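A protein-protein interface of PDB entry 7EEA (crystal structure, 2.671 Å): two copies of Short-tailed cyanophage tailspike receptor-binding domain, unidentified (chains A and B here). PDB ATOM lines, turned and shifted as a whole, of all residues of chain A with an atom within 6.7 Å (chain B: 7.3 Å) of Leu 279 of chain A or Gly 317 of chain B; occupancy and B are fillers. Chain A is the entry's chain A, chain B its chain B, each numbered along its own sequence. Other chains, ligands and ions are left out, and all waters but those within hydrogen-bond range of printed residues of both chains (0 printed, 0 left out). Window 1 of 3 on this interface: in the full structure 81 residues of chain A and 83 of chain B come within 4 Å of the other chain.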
ATOM      1  N   PHE A 253       5.023  32.705 -31.194  1.00  0.00           N
ATOM      2  CA  PHE A 253       4.709  32.531 -29.782  1.00  0.00           C
ATOM      3  C   PHE A 253       5.868  31.945 -28.995  1.00  0.00           C
ATOM      4  O   PHE A 253       6.221  32.474 -27.933  1.00  0.00           O
ATOM      5  CB  PHE A 253       3.470  31.639 -29.610  1.00  0.00           C
ATOM      6  CG  PHE A 253       3.217  31.239 -28.179  1.00  0.00           C
ATOM      7  CD1 PHE A 253       2.755  32.165 -27.258  1.00  0.00           C
ATOM      8  CD2 PHE A 253       3.464  29.943 -27.751  1.00  0.00           C
ATOM      9  CE1 PHE A 253       2.529  31.807 -25.942  1.00  0.00           C
ATOM     10  CE2 PHE A 253       3.244  29.579 -26.437  1.00  0.00           C
ATOM     11  CZ  PHE A 253       2.774  30.513 -25.530  1.00  0.00           C
ATOM     12  N   GLY A 254       6.459  30.853 -29.470  1.00  0.00           N
ATOM     13  CA  GLY A 254       7.522  30.201 -28.737  1.00  0.00           C
ATOM     14  C   GLY A 254       7.381  28.694 -28.696  1.00  0.00           C
ATOM     15  O   GLY A 254       7.268  28.045 -29.738  1.00  0.00           O
ATOM     16  N   VAL A 255       7.374  28.126 -27.493  1.00  0.00           N
ATOM     17  CA  VAL A 255       7.439  26.684 -27.300  1.00  0.00           C
ATOM     18  C   VAL A 255       6.169  26.207 -26.610  1.00  0.00           C
ATOM     19  O   VAL A 255       5.681  26.843 -25.666  1.00  0.00           O
ATOM     20  CB  VAL A 255       8.694  26.287 -26.491  1.00  0.00           C
ATOM     21  CG1 VAL A 255       8.770  27.069 -25.183  1.00  0.00           C
ATOM     22  CG2 VAL A 255       8.721  24.787 -26.239  1.00  0.00           C
ATOM     23  N   LYS A 256       5.628  25.089 -27.096  1.00  0.00           N
ATOM     24  CA  LYS A 256       4.468  24.430 -26.509  1.00  0.00           C
ATOM     25  C   LYS A 256       4.807  22.967 -26.265  1.00  0.00           C
ATOM     26  O   LYS A 256       5.278  22.279 -27.174  1.00  0.00           O
ATOM     27  CB  LYS A 256       3.242  24.531 -27.422  1.00  0.00           C
ATOM     28  CG  LYS A 256       2.800  25.944 -27.737  1.00  0.00           C
ATOM     29  CD  LYS A 256       1.569  25.931 -28.628  1.00  0.00           C
ATOM     30  CE  LYS A 256       1.139  27.340 -28.999  1.00  0.00           C
ATOM     31  NZ  LYS A 256      -0.057  27.334 -29.885  1.00  0.00           N
ATOM     32  N   ILE A 257       4.568  22.495 -25.045  1.00  0.00           N
ATOM     33  CA  ILE A 257       4.843  21.113 -24.661  1.00  0.00           C
ATOM     34  C   ILE A 257       3.561  20.533 -24.076  1.00  0.00           C
ATOM     35  O   ILE A 257       3.083  21.003 -23.035  1.00  0.00           O
ATOM     36  CB  ILE A 257       6.007  21.022 -23.659  1.00  0.00           C
ATOM     37  CG1 ILE A 257       7.246  21.716 -24.235  1.00  0.00           C
ATOM     38  CG2 ILE A 257       6.321  19.573 -23.333  1.00  0.00           C
ATOM     39  CD1 ILE A 257       8.330  21.998 -23.221  1.00  0.00           C
ATOM     40  N   ASN A 258       3.010  19.512 -24.736  1.00  0.00           N
ATOM     41  CA  ASN A 258       1.627  19.112 -24.508  1.00  0.00           C
ATOM     42  C   ASN A 258       1.460  17.827 -23.709  1.00  0.00           C
ATOM     43  O   ASN A 258       0.424  17.655 -23.058  1.00  0.00           O
ATOM     44  CB  ASN A 258       0.902  18.943 -25.845  1.00  0.00           C
ATOM     45  CG  ASN A 258       0.562  20.267 -26.490  1.00  0.00           C
ATOM     46  OD1 ASN A 258       0.350  20.346 -27.700  1.00  0.00           O
ATOM     47  ND2 ASN A 258       0.508  21.321 -25.683  1.00  0.00           N
ATOM     48  N   GLY A 277       7.118  33.111 -25.201  1.00  0.00           N
ATOM     49  CA  GLY A 277       5.978  32.386 -24.674  1.00  0.00           C
ATOM     50  C   GLY A 277       6.280  30.932 -24.373  1.00  0.00           C
ATOM     51  O   GLY A 277       6.939  30.250 -25.162  1.00  0.00           O
ATOM     52  N   VAL A 278       5.805  30.449 -23.228  1.00  0.00           N
ATOM     53  CA  VAL A 278       6.003  29.067 -22.807  1.00  0.00           C
ATOM     54  C   VAL A 278       4.652  28.495 -22.399  1.00  0.00           C
ATOM     55  O   VAL A 278       3.979  29.047 -21.521  1.00  0.00           O
ATOM     56  CB  VAL A 278       7.008  28.949 -21.650  1.00  0.00           C
ATOM     57  CG1 VAL A 278       7.175  27.498 -21.241  1.00  0.00           C
ATOM     58  CG2 VAL A 278       8.340  29.545 -22.044  1.00  0.00           C
ATOM     59  N   LEU A 279       4.262  27.391 -23.033  1.00  0.00           N
ATOM     60  CA  LEU A 279       3.037  26.663 -22.712  1.00  0.00           C
ATOM     61  C   LEU A 279       3.415  25.216 -22.426  1.00  0.00           C
ATOM     62  O   LEU A 279       3.800  24.478 -23.340  1.00  0.00           O
ATOM     63  CB  LEU A 279       2.029  26.749 -23.859  1.00  0.00           C
ATOM     64  CG  LEU A 279       0.674  27.409 -23.606  1.00  0.00           C
ATOM     65  CD1 LEU A 279      -0.257  27.168 -24.786  1.00  0.00           C
ATOM     66  CD2 LEU A 279       0.051  26.896 -22.313  1.00  0.00           C
ATOM     67  N   ILE A 280       3.313  24.812 -21.164  1.00  0.00           N
ATOM     68  CA  ILE A 280       3.605  23.447 -20.740  1.00  0.00           C
ATOM     69  C   ILE A 280       2.360  22.901 -20.061  1.00  0.00           C
ATOM     70  O   ILE A 280       1.953  23.402 -19.008  1.00  0.00           O
ATOM     71  CB  ILE A 280       4.821  23.388 -19.803  1.00  0.00           C
ATOM     72  CG1 ILE A 280       6.056  23.967 -20.498  1.00  0.00           C
ATOM     73  CG2 ILE A 280       5.079  21.960 -19.356  1.00  0.00           C
ATOM     74  CD1 ILE A 280       7.220  24.221 -19.565  1.00  0.00           C
ATOM     75  N   GLN A 281       1.757  21.877 -20.655  1.00  0.00           N
ATOM     76  CA  GLN A 281       0.475  21.365 -20.193  1.00  0.00           C
ATOM     77  C   GLN A 281       0.528  19.848 -20.093  1.00  0.00           C
ATOM     78  O   GLN A 281       1.008  19.182 -21.013  1.00  0.00           O
ATOM     79  CB  GLN A 281      -0.649  21.797 -21.138  1.00  0.00           C
ATOM     80  CG  GLN A 281      -2.028  21.821 -20.504  1.00  0.00           C
ATOM     81  CD  GLN A 281      -2.312  23.115 -19.761  1.00  0.00           C
ATOM     82  OE1 GLN A 281      -1.546  24.080 -19.848  1.00  0.00           O
ATOM     83  NE2 GLN A 281      -3.420  23.143 -19.026  1.00  0.00           N
ATOM     84  N   LEU A 312       6.151  34.952 -21.115  1.00  0.00           N
ATOM     85  CA  LEU A 312       4.849  34.421 -20.743  1.00  0.00           C
ATOM     86  C   LEU A 312       5.016  32.953 -20.391  1.00  0.00           C
ATOM     87  O   LEU A 312       5.558  32.183 -21.186  1.00  0.00           O
ATOM     88  CB  LEU A 312       3.843  34.581 -21.890  1.00  0.00           C
ATOM     89  CG  LEU A 312       2.346  34.514 -21.599  1.00  0.00           C
ATOM     90  CD1 LEU A 312       1.606  35.219 -22.712  1.00  0.00           C
ATOM     91  CD2 LEU A 312       1.863  33.077 -21.477  1.00  0.00           C
ATOM     92  N   VAL A 313       4.557  32.569 -19.203  1.00  0.00           N
ATOM     93  CA  VAL A 313       4.658  31.190 -18.739  1.00  0.00           C
ATOM     94  C   VAL A 313       3.285  30.734 -18.268  1.00  0.00           C
ATOM     95  O   VAL A 313       2.647  31.406 -17.450  1.00  0.00           O
ATOM     96  CB  VAL A 313       5.698  31.034 -17.614  1.00  0.00           C
ATOM     97  CG1 VAL A 313       5.680  29.612 -17.071  1.00  0.00           C
ATOM     98  CG2 VAL A 313       7.079  31.391 -18.128  1.00  0.00           C
ATOM     99  N   ASP A 314       2.835  29.597 -18.793  1.00  0.00           N
ATOM    100  CA  ASP A 314       1.567  28.981 -18.404  1.00  0.00           C
ATOM    101  C   ASP A 314       1.821  27.480 -18.343  1.00  0.00           C
ATOM    102  O   ASP A 314       1.807  26.802 -19.374  1.00  0.00           O
ATOM    103  CB  ASP A 314       0.456  29.325 -19.392  1.00  0.00           C
ATOM    104  CG  ASP A 314      -0.908  28.799 -18.965  1.00  0.00           C
ATOM    105  OD1 ASP A 314      -0.978  27.828 -18.180  1.00  0.00           O
ATOM    106  OD2 ASP A 314      -1.923  29.365 -19.427  1.00  0.00           O
ATOM    107  N   ILE A 315       2.064  26.965 -17.143  1.00  0.00           N
ATOM    108  CA  ILE A 315       2.206  25.530 -16.933  1.00  0.00           C
ATOM    109  C   ILE A 315       1.039  25.055 -16.077  1.00  0.00           C
ATOM    110  O   ILE A 315       0.693  25.682 -15.069  1.00  0.00           O
ATOM    111  CB  ILE A 315       3.575  25.162 -16.327  1.00  0.00           C
ATOM    112  CG1 ILE A 315       3.596  25.285 -14.809  1.00  0.00           C
ATOM    113  CG2 ILE A 315       4.681  26.019 -16.937  1.00  0.00           C
ATOM    114  CD1 ILE A 315       4.670  24.446 -14.178  1.00  0.00           C
ATOM    115  N   GLY A 316       0.401  23.981 -16.515  1.00  0.00           N
ATOM    116  CA  GLY A 316      -0.790  23.481 -15.855  1.00  0.00           C
ATOM    117  C   GLY A 316      -0.959  22.001 -16.099  1.00  0.00           C
ATOM    118  O   GLY A 316      -0.556  21.474 -17.141  1.00  0.00           O
ATOM    119  N   GLN A 348       1.918  37.180 -18.079  1.00  0.00           N
ATOM    120  CA  GLN A 348       1.519  36.392 -16.924  1.00  0.00           C
ATOM    121  C   GLN A 348       2.486  35.247 -16.660  1.00  0.00           C
ATOM    122  O   GLN A 348       3.102  34.690 -17.575  1.00  0.00           O
ATOM    123  CB  GLN A 348       0.117  35.825 -17.135  1.00  0.00           C
ATOM    124  CG  GLN A 348       0.045  34.809 -18.267  1.00  0.00           C
ATOM    125  CD  GLN A 348      -1.369  34.531 -18.726  1.00  0.00           C
ATOM    126  OE1 GLN A 348      -1.589  33.748 -19.652  1.00  0.00           O
ATOM    127  NE2 GLN A 348      -2.341  35.156 -18.070  1.00  0.00           N
ATOM    128  N   HIS A 352      -0.573  26.458 -12.298  1.00  0.00           N
ATOM    129  CA  HIS A 352      -1.888  26.059 -11.825  1.00  0.00           C
ATOM    130  C   HIS A 352      -2.117  24.576 -12.066  1.00  0.00           C
ATOM    131  O   HIS A 352      -1.609  24.006 -13.032  1.00  0.00           O
ATOM    132  CB  HIS A 352      -2.996  26.870 -12.512  1.00  0.00           C
ATOM    133  CG  HIS A 352      -3.065  26.671 -13.994  1.00  0.00           C
ATOM    134  ND1 HIS A 352      -3.951  25.797 -14.587  1.00  0.00           N
ATOM    135  CD2 HIS A 352      -2.362  27.236 -15.005  1.00  0.00           C
ATOM    136  CE1 HIS A 352      -3.791  25.833 -15.898  1.00  0.00           C
ATOM    137  NE2 HIS A 352      -2.832  26.699 -16.177  1.00  0.00           N
ATOM    138  N   GLY B 259      -5.403  23.851 -30.200  1.00  0.00           N
ATOM    139  CA  GLY B 259      -4.142  24.560 -30.266  1.00  0.00           C
ATOM    140  C   GLY B 259      -3.930  25.305 -31.565  1.00  0.00           C
ATOM    141  O   GLY B 259      -4.799  26.069 -32.002  1.00  0.00           O
ATOM    142  N   ILE B 280     -12.199  25.795 -26.616  1.00  0.00           N
ATOM    143  CA  ILE B 280     -11.011  26.376 -27.234  1.00  0.00           C
ATOM    144  C   ILE B 280      -9.900  26.340 -26.196  1.00  0.00           C
ATOM    145  O   ILE B 280      -9.978  27.032 -25.173  1.00  0.00           O
ATOM    146  CB  ILE B 280     -11.259  27.808 -27.730  1.00  0.00           C
ATOM    147  CG1 ILE B 280     -12.459  27.851 -28.679  1.00  0.00           C
ATOM    148  CG2 ILE B 280     -10.022  28.355 -28.420  1.00  0.00           C
ATOM    149  CD1 ILE B 280     -12.891  29.258 -29.052  1.00  0.00           C
ATOM    150  N   GLN B 281      -8.863  25.546 -26.449  1.00  0.00           N
ATOM    151  CA  GLN B 281      -7.813  25.315 -25.466  1.00  0.00           C
ATOM    152  C   GLN B 281      -6.439  25.514 -26.089  1.00  0.00           C
ATOM    153  O   GLN B 281      -6.119  24.891 -27.107  1.00  0.00           O
ATOM    154  CB  GLN B 281      -7.922  23.904 -24.877  1.00  0.00           C
ATOM    155  CG  GLN B 281      -7.300  23.756 -23.499  1.00  0.00           C
ATOM    156  CD  GLN B 281      -8.163  24.348 -22.401  1.00  0.00           C
ATOM    157  OE1 GLN B 281      -9.395  24.290 -22.461  1.00  0.00           O
ATOM    158  NE2 GLN B 281      -7.520  24.924 -21.390  1.00  0.00           N
ATOM    159  N   GLY B 282      -5.631  26.375 -25.473  1.00  0.00           N
ATOM    160  CA  GLY B 282      -4.230  26.501 -25.838  1.00  0.00           C
ATOM    161  C   GLY B 282      -3.953  27.080 -27.207  1.00  0.00           C
ATOM    162  O   GLY B 282      -2.929  26.751 -27.813  1.00  0.00           O
ATOM    163  N   VAL B 283      -4.828  27.938 -27.709  1.00  0.00           N
ATOM    164  CA  VAL B 283      -4.670  28.539 -29.028  1.00  0.00           C
ATOM    165  C   VAL B 283      -3.864  29.823 -28.895  1.00  0.00           C
ATOM    166  O   VAL B 283      -4.077  30.610 -27.968  1.00  0.00           O
ATOM    167  CB  VAL B 283      -6.047  28.801 -29.669  1.00  0.00           C
ATOM    168  CG1 VAL B 283      -5.897  29.504 -31.010  1.00  0.00           C
ATOM    169  CG2 VAL B 283      -6.808  27.498 -29.830  1.00  0.00           C
ATOM    170  N   THR B 284      -2.930  30.041 -29.818  1.00  0.00           N
ATOM    171  CA  THR B 284      -2.112  31.247 -29.812  1.00  0.00           C
ATOM    172  C   THR B 284      -2.226  31.947 -31.158  1.00  0.00           C
ATOM    173  O   THR B 284      -2.132  31.303 -32.207  1.00  0.00           O
ATOM    174  CB  THR B 284      -0.645  30.931 -29.501  1.00  0.00           C
ATOM    175  OG1 THR B 284      -0.160  29.934 -30.411  1.00  0.00           O
ATOM    176  CG2 THR B 284      -0.501  30.425 -28.069  1.00  0.00           C
ATOM    177  N   ASP B 314     -15.951  27.319 -23.167  1.00  0.00           N
ATOM    178  CA  ASP B 314     -14.794  27.128 -22.293  1.00  0.00           C
ATOM    179  C   ASP B 314     -13.555  27.425 -23.132  1.00  0.00           C
ATOM    180  O   ASP B 314     -13.161  26.619 -23.979  1.00  0.00           O
ATOM    181  CB  ASP B 314     -14.759  25.718 -21.711  1.00  0.00           C
ATOM    182  CG  ASP B 314     -13.585  25.495 -20.766  1.00  0.00           C
ATOM    183  OD1 ASP B 314     -12.794  26.439 -20.541  1.00  0.00           O
ATOM    184  OD2 ASP B 314     -13.449  24.367 -20.248  1.00  0.00           O
ATOM    185  N   ILE B 315     -12.952  28.587 -22.903  1.00  0.00           N
ATOM    186  CA  ILE B 315     -11.711  28.961 -23.567  1.00  0.00           C
ATOM    187  C   ILE B 315     -10.644  29.164 -22.495  1.00  0.00           C
ATOM    188  O   ILE B 315     -10.857  29.891 -21.520  1.00  0.00           O
ATOM    189  CB  ILE B 315     -11.883  30.203 -24.467  1.00  0.00           C
ATOM    190  CG1 ILE B 315     -12.037  31.489 -23.668  1.00  0.00           C
ATOM    191  CG2 ILE B 315     -13.095  30.042 -25.377  1.00  0.00           C
ATOM    192  CD1 ILE B 315     -11.666  32.701 -24.467  1.00  0.00           C
ATOM    193  N   GLY B 316      -9.522  28.482 -22.654  1.00  0.00           N
ATOM    194  CA  GLY B 316      -8.485  28.489 -21.636  1.00  0.00           C
ATOM    195  C   GLY B 316      -7.112  28.309 -22.240  1.00  0.00           C
ATOM    196  O   GLY B 316      -6.947  27.658 -23.277  1.00  0.00           O
ATOM    197  N   GLY B 317      -6.114  28.891 -21.579  1.00  0.00           N
ATOM    198  CA  GLY B 317      -4.743  28.761 -22.030  1.00  0.00           C
ATOM    199  C   GLY B 317      -4.462  29.393 -23.370  1.00  0.00           C
ATOM    200  O   GLY B 317      -3.490  29.018 -24.031  1.00  0.00           O
ATOM    201  N   CYS B 318      -5.282  30.350 -23.792  1.00  0.00           N
ATOM    202  CA  CYS B 318      -5.137  30.988 -25.092  1.00  0.00           C
ATOM    203  C   CYS B 318      -4.342  32.280 -24.954  1.00  0.00           C
ATOM    204  O   CYS B 318      -4.659  33.124 -24.110  1.00  0.00           O
ATOM    205  CB  CYS B 318      -6.507  31.263 -25.715  1.00  0.00           C
ATOM    206  SG  CYS B 318      -7.372  29.772 -26.256  1.00  0.00           S
ATOM    207  N   LYS B 319      -3.311  32.429 -25.784  1.00  0.00           N
ATOM    208  CA  LYS B 319      -2.413  33.579 -25.742  1.00  0.00           C
ATOM    209  C   LYS B 319      -2.566  34.350 -27.046  1.00  0.00           C
ATOM    210  O   LYS B 319      -2.107  33.895 -28.099  1.00  0.00           O
ATOM    211  CB  LYS B 319      -0.969  33.132 -25.526  1.00  0.00           C
ATOM    212  CG  LYS B 319      -0.826  31.925 -24.612  1.00  0.00           C
ATOM    213  CD  LYS B 319      -1.294  32.228 -23.194  1.00  0.00           C
ATOM    214  CE  LYS B 319      -1.346  30.963 -22.346  1.00  0.00           C
ATOM    215  NZ  LYS B 319      -1.792  31.243 -20.952  1.00  0.00           N
ATOM    216  N   LEU B 320      -3.210  35.513 -26.975  1.00  0.00           N
ATOM    217  CA  LEU B 320      -3.568  36.306 -28.148  1.00  0.00           C
ATOM    218  C   LEU B 320      -2.772  37.602 -28.110  1.00  0.00           C
ATOM    219  O   LEU B 320      -3.028  38.465 -27.263  1.00  0.00           O
ATOM    220  CB  LEU B 320      -5.071  36.591 -28.176  1.00  0.00           C
ATOM    221  CG  LEU B 320      -6.071  35.536 -28.663  1.00  0.00           C
ATOM    222  CD1 LEU B 320      -5.804  34.152 -28.088  1.00  0.00           C
ATOM    223  CD2 LEU B 320      -7.474  35.981 -28.306  1.00  0.00           C
ATOM    224  N   VAL B 351     -13.959  31.738 -19.026  1.00  0.00           N
ATOM    225  CA  VAL B 351     -12.807  32.354 -19.670  1.00  0.00           C
ATOM    226  C   VAL B 351     -11.699  32.374 -18.628  1.00  0.00           C
ATOM    227  O   VAL B 351     -11.737  33.184 -17.691  1.00  0.00           O
ATOM    228  CB  VAL B 351     -13.117  33.765 -20.185  1.00  0.00           C
ATOM    229  CG1 VAL B 351     -11.924  34.328 -20.933  1.00  0.00           C
ATOM    230  CG2 VAL B 351     -14.351  33.747 -21.072  1.00  0.00           C
ATOM    231  N   HIS B 352     -10.719  31.484 -18.777  1.00  0.00           N
ATOM    232  CA  HIS B 352      -9.718  31.292 -17.738  1.00  0.00           C
ATOM    233  C   HIS B 352      -8.336  31.078 -18.341  1.00  0.00           C
ATOM    234  O   HIS B 352      -8.189  30.475 -19.405  1.00  0.00           O
ATOM    235  CB  HIS B 352     -10.078  30.106 -16.833  1.00  0.00           C
ATOM    236  CG  HIS B 352     -10.206  28.803 -17.561  1.00  0.00           C
ATOM    237  ND1 HIS B 352      -9.305  27.773 -17.403  1.00  0.00           N
ATOM    238  CD2 HIS B 352     -11.136  28.359 -18.439  1.00  0.00           C
ATOM    239  CE1 HIS B 352      -9.671  26.751 -18.156  1.00  0.00           C
ATOM    240  NE2 HIS B 352     -10.779  27.081 -18.795  1.00  0.00           N
ATOM    241  N   ASP B 353      -7.321  31.589 -17.637  1.00  0.00           N
ATOM    242  CA  ASP B 353      -5.911  31.344 -17.952  1.00  0.00           C
ATOM    243  C   ASP B 353      -5.529  31.827 -19.350  1.00  0.00           C
ATOM    244  O   ASP B 353      -4.657  31.246 -20.000  1.00  0.00           O
ATOM    245  CB  ASP B 353      -5.561  29.861 -17.790  1.00  0.00           C
ATOM    246  CG  ASP B 353      -5.873  29.338 -16.403  1.00  0.00           C
ATOM    247  OD1 ASP B 353      -5.205  29.769 -15.438  1.00  0.00           O
ATOM    248  OD2 ASP B 353      -6.790  28.501 -16.274  1.00  0.00           O
ATOM    249  N   ASN B 354      -6.160  32.899 -19.821  1.00  0.00           N
ATOM    250  CA  ASN B 354      -5.822  33.492 -21.105  1.00  0.00           C
ATOM    251  C   ASN B 354      -5.027  34.777 -20.908  1.00  0.00           C
ATOM    252  O   ASN B 354      -5.073  35.411 -19.850  1.00  0.00           O
ATOM    253  CB  ASN B 354      -7.083  33.780 -21.926  1.00  0.00           C
ATOM    254  CG  ASN B 354      -7.993  32.579 -22.033  1.00  0.00           C
ATOM    255  OD1 ASN B 354      -7.687  31.614 -22.733  1.00  0.00           O
ATOM    256  ND2 ASN B 354      -9.123  32.631 -21.338  1.00  0.00           N
ATOM    257  N   GLN B 355      -4.288  35.153 -21.950  1.00  0.00           N
ATOM    258  CA  GLN B 355      -3.506  36.379 -21.956  1.00  0.00           C
ATOM    259  C   GLN B 355      -3.777  37.159 -23.233  1.00  0.00           C
ATOM    260  O   GLN B 355      -3.856  36.579 -24.320  1.00  0.00           O
ATOM    261  CB  GLN B 355      -2.006  36.094 -21.838  1.00  0.00           C
ATOM    262  CG  GLN B 355      -1.134  37.289 -22.172  1.00  0.00           C
ATOM    263  CD  GLN B 355      -0.888  38.175 -20.972  1.00  0.00           C
ATOM    264  OE1 GLN B 355      -1.210  39.365 -20.985  1.00  0.00           O
ATOM    265  NE2 GLN B 355      -0.319  37.600 -19.922  1.00  0.00           N
ATOM    266  N   ASN B 385      -7.020  35.425 -15.712  1.00  0.00           N
ATOM    267  CA  ASN B 385      -6.651  36.007 -16.991  1.00  0.00           C
ATOM    268  C   ASN B 385      -5.819  37.263 -16.764  1.00  0.00           C
ATOM    269  O   ASN B 385      -5.823  37.856 -15.682  1.00  0.00           O
ATOM    270  CB  ASN B 385      -7.894  36.340 -17.821  1.00  0.00           C
ATOM    271  CG  ASN B 385      -8.749  35.121 -18.104  1.00  0.00           C
ATOM    272  OD1 ASN B 385      -8.452  34.333 -19.002  1.00  0.00           O
ATOM    273  ND2 ASN B 385      -9.816  34.958 -17.332  1.00  0.00           N
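The side-chain hydroxyl (OG1) of Thr 284 of chain B is in hydrogen-bond range of the side-chain amino group (NZ) of Lys 256 of chain A (2.7 Å). The side-chain carboxylate (OD2) of Asp 314 of chain A is in salt-bridge range of the side-chain amino group (NZ) of Lys 319 of chain B, at 2.4 Å. NZ of Lys 319 of chain B lies within hydrogen-bond range of OE1 of Gln 348 of chain A (2.8 Å). The side-chain amide nitrogen (NE2) of Gln 348 of chain A sits at hydrogen-bond distance from the backbone carbonyl oxygen (O) of Asn 354 of chain B, at 3.3 Å. N of Gln 348 of chain A lies close to NE2 of Gln 355 of chain B, at 2.9 Å. OD2 of Asp 314 of chain A sits close to O of Asp 353 of chain B, at 3.4 Å.
The backbone NH (N) of Leu 279 of chain A is in hydrogen-bond range of the backbone carbonyl oxygen (O) of Val 255 of chain A, at 3.0 Å. The backbone NH of Ile 280 of chain A sits at hydrogen-bond distance from the backbone carbonyl oxygen of Asp 314 of chain A (3.1 Å). The backbone NH (N) of Val 313 of chain A lies within hydrogen-bond range of the backbone carbonyl oxygen (O) of Gln 348 of chain A, 3.0 Å away. The backbone carbonyl oxygen (O) of Ile 315 of chain A sits at hydrogen-bond distance from the backbone NH (N) of His 352 of chain A. N of Asp 353 of chain B lies within hydrogen-bond range of OD1 of Asn 385 of chain B, at 3.3 Å. The backbone NH (N) of Asn 354 of chain B is in hydrogen-bond range of the side-chain amide oxygen (OD1) of Asn 385 of chain B.
Among the printed residues, merely in contact across the chains: Phe 253 of chain A with Thr 284 of chain B, Phe 253 of chain A with Lys 319 of chain B, Lys 256 of chain A with Gly 282 of chain B, Leu 279 of chain A with Gly 317 of chain B, Leu 312 of chain A with Lys 319 of chain B, Leu 312 of chain A with Gln 355 of chain B, Asp 314 of chain A with Gly 317 of chain B, Gln 348 of chain A with Asp 353 of chain B and His 352 of chain A with Asp 353 of chain B.
Of the printed residues of chain B, Phe 253 of chain A touches Thr 284 (3.8 Å) and Lys 319 (3.6 Å). Leu 279 of chain A touches just one residue of chain B: Gly 317. Of the printed residues of chain B, Asp 314 of chain A touches Gly 317, Lys 319 and Asp 353. Printed residues of chain A within 4 Å of Gly 282 of chain B: Lys 256. Of the printed residues of chain A, Thr 284 of chain B touches Phe 253 and Lys 256. Gly 317 of chain B touches just these residues of chain A: Leu 279 (3.8 Å) and Asp 314 (3.9 Å). Printed residues of chain A within 4 Å of Lys 319 of chain B: Phe 253, Leu 312, Asp 314 and Gln 348. Leu 320 of chain B touches none of the printed residues of chain A. The nearest residue of chain A that does not touch Gly 317 of chain B is Gln 281 of chain A (6.1 Å). The nearest printed residue of chain B that does not touch Asp 314 of chain A is Asn 354 of chain B (5.5 Å).
Printed residues of chain B that touch a printed residue of chain A: Gly 282, Thr 284, Gly 317, Lys 319, Asp 353, Asn 354 and Gln 355. Hydrophobic or aromatic side chains of chain A that line the printed part of chain B: Phe 253, Leu 279, Leu 312 and His 352. Along chain A the printed residues that touch a printed residue of chain B span positions 253 to 352. Among the printed residues, 15 pairs touch across the chains.
Positions printed for both chains: 280, 281, 314, 315, 316 and 352. Of the 15 pairs that touch across the chains among the printed residues, none has its exchanged pair printed and touching as well.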
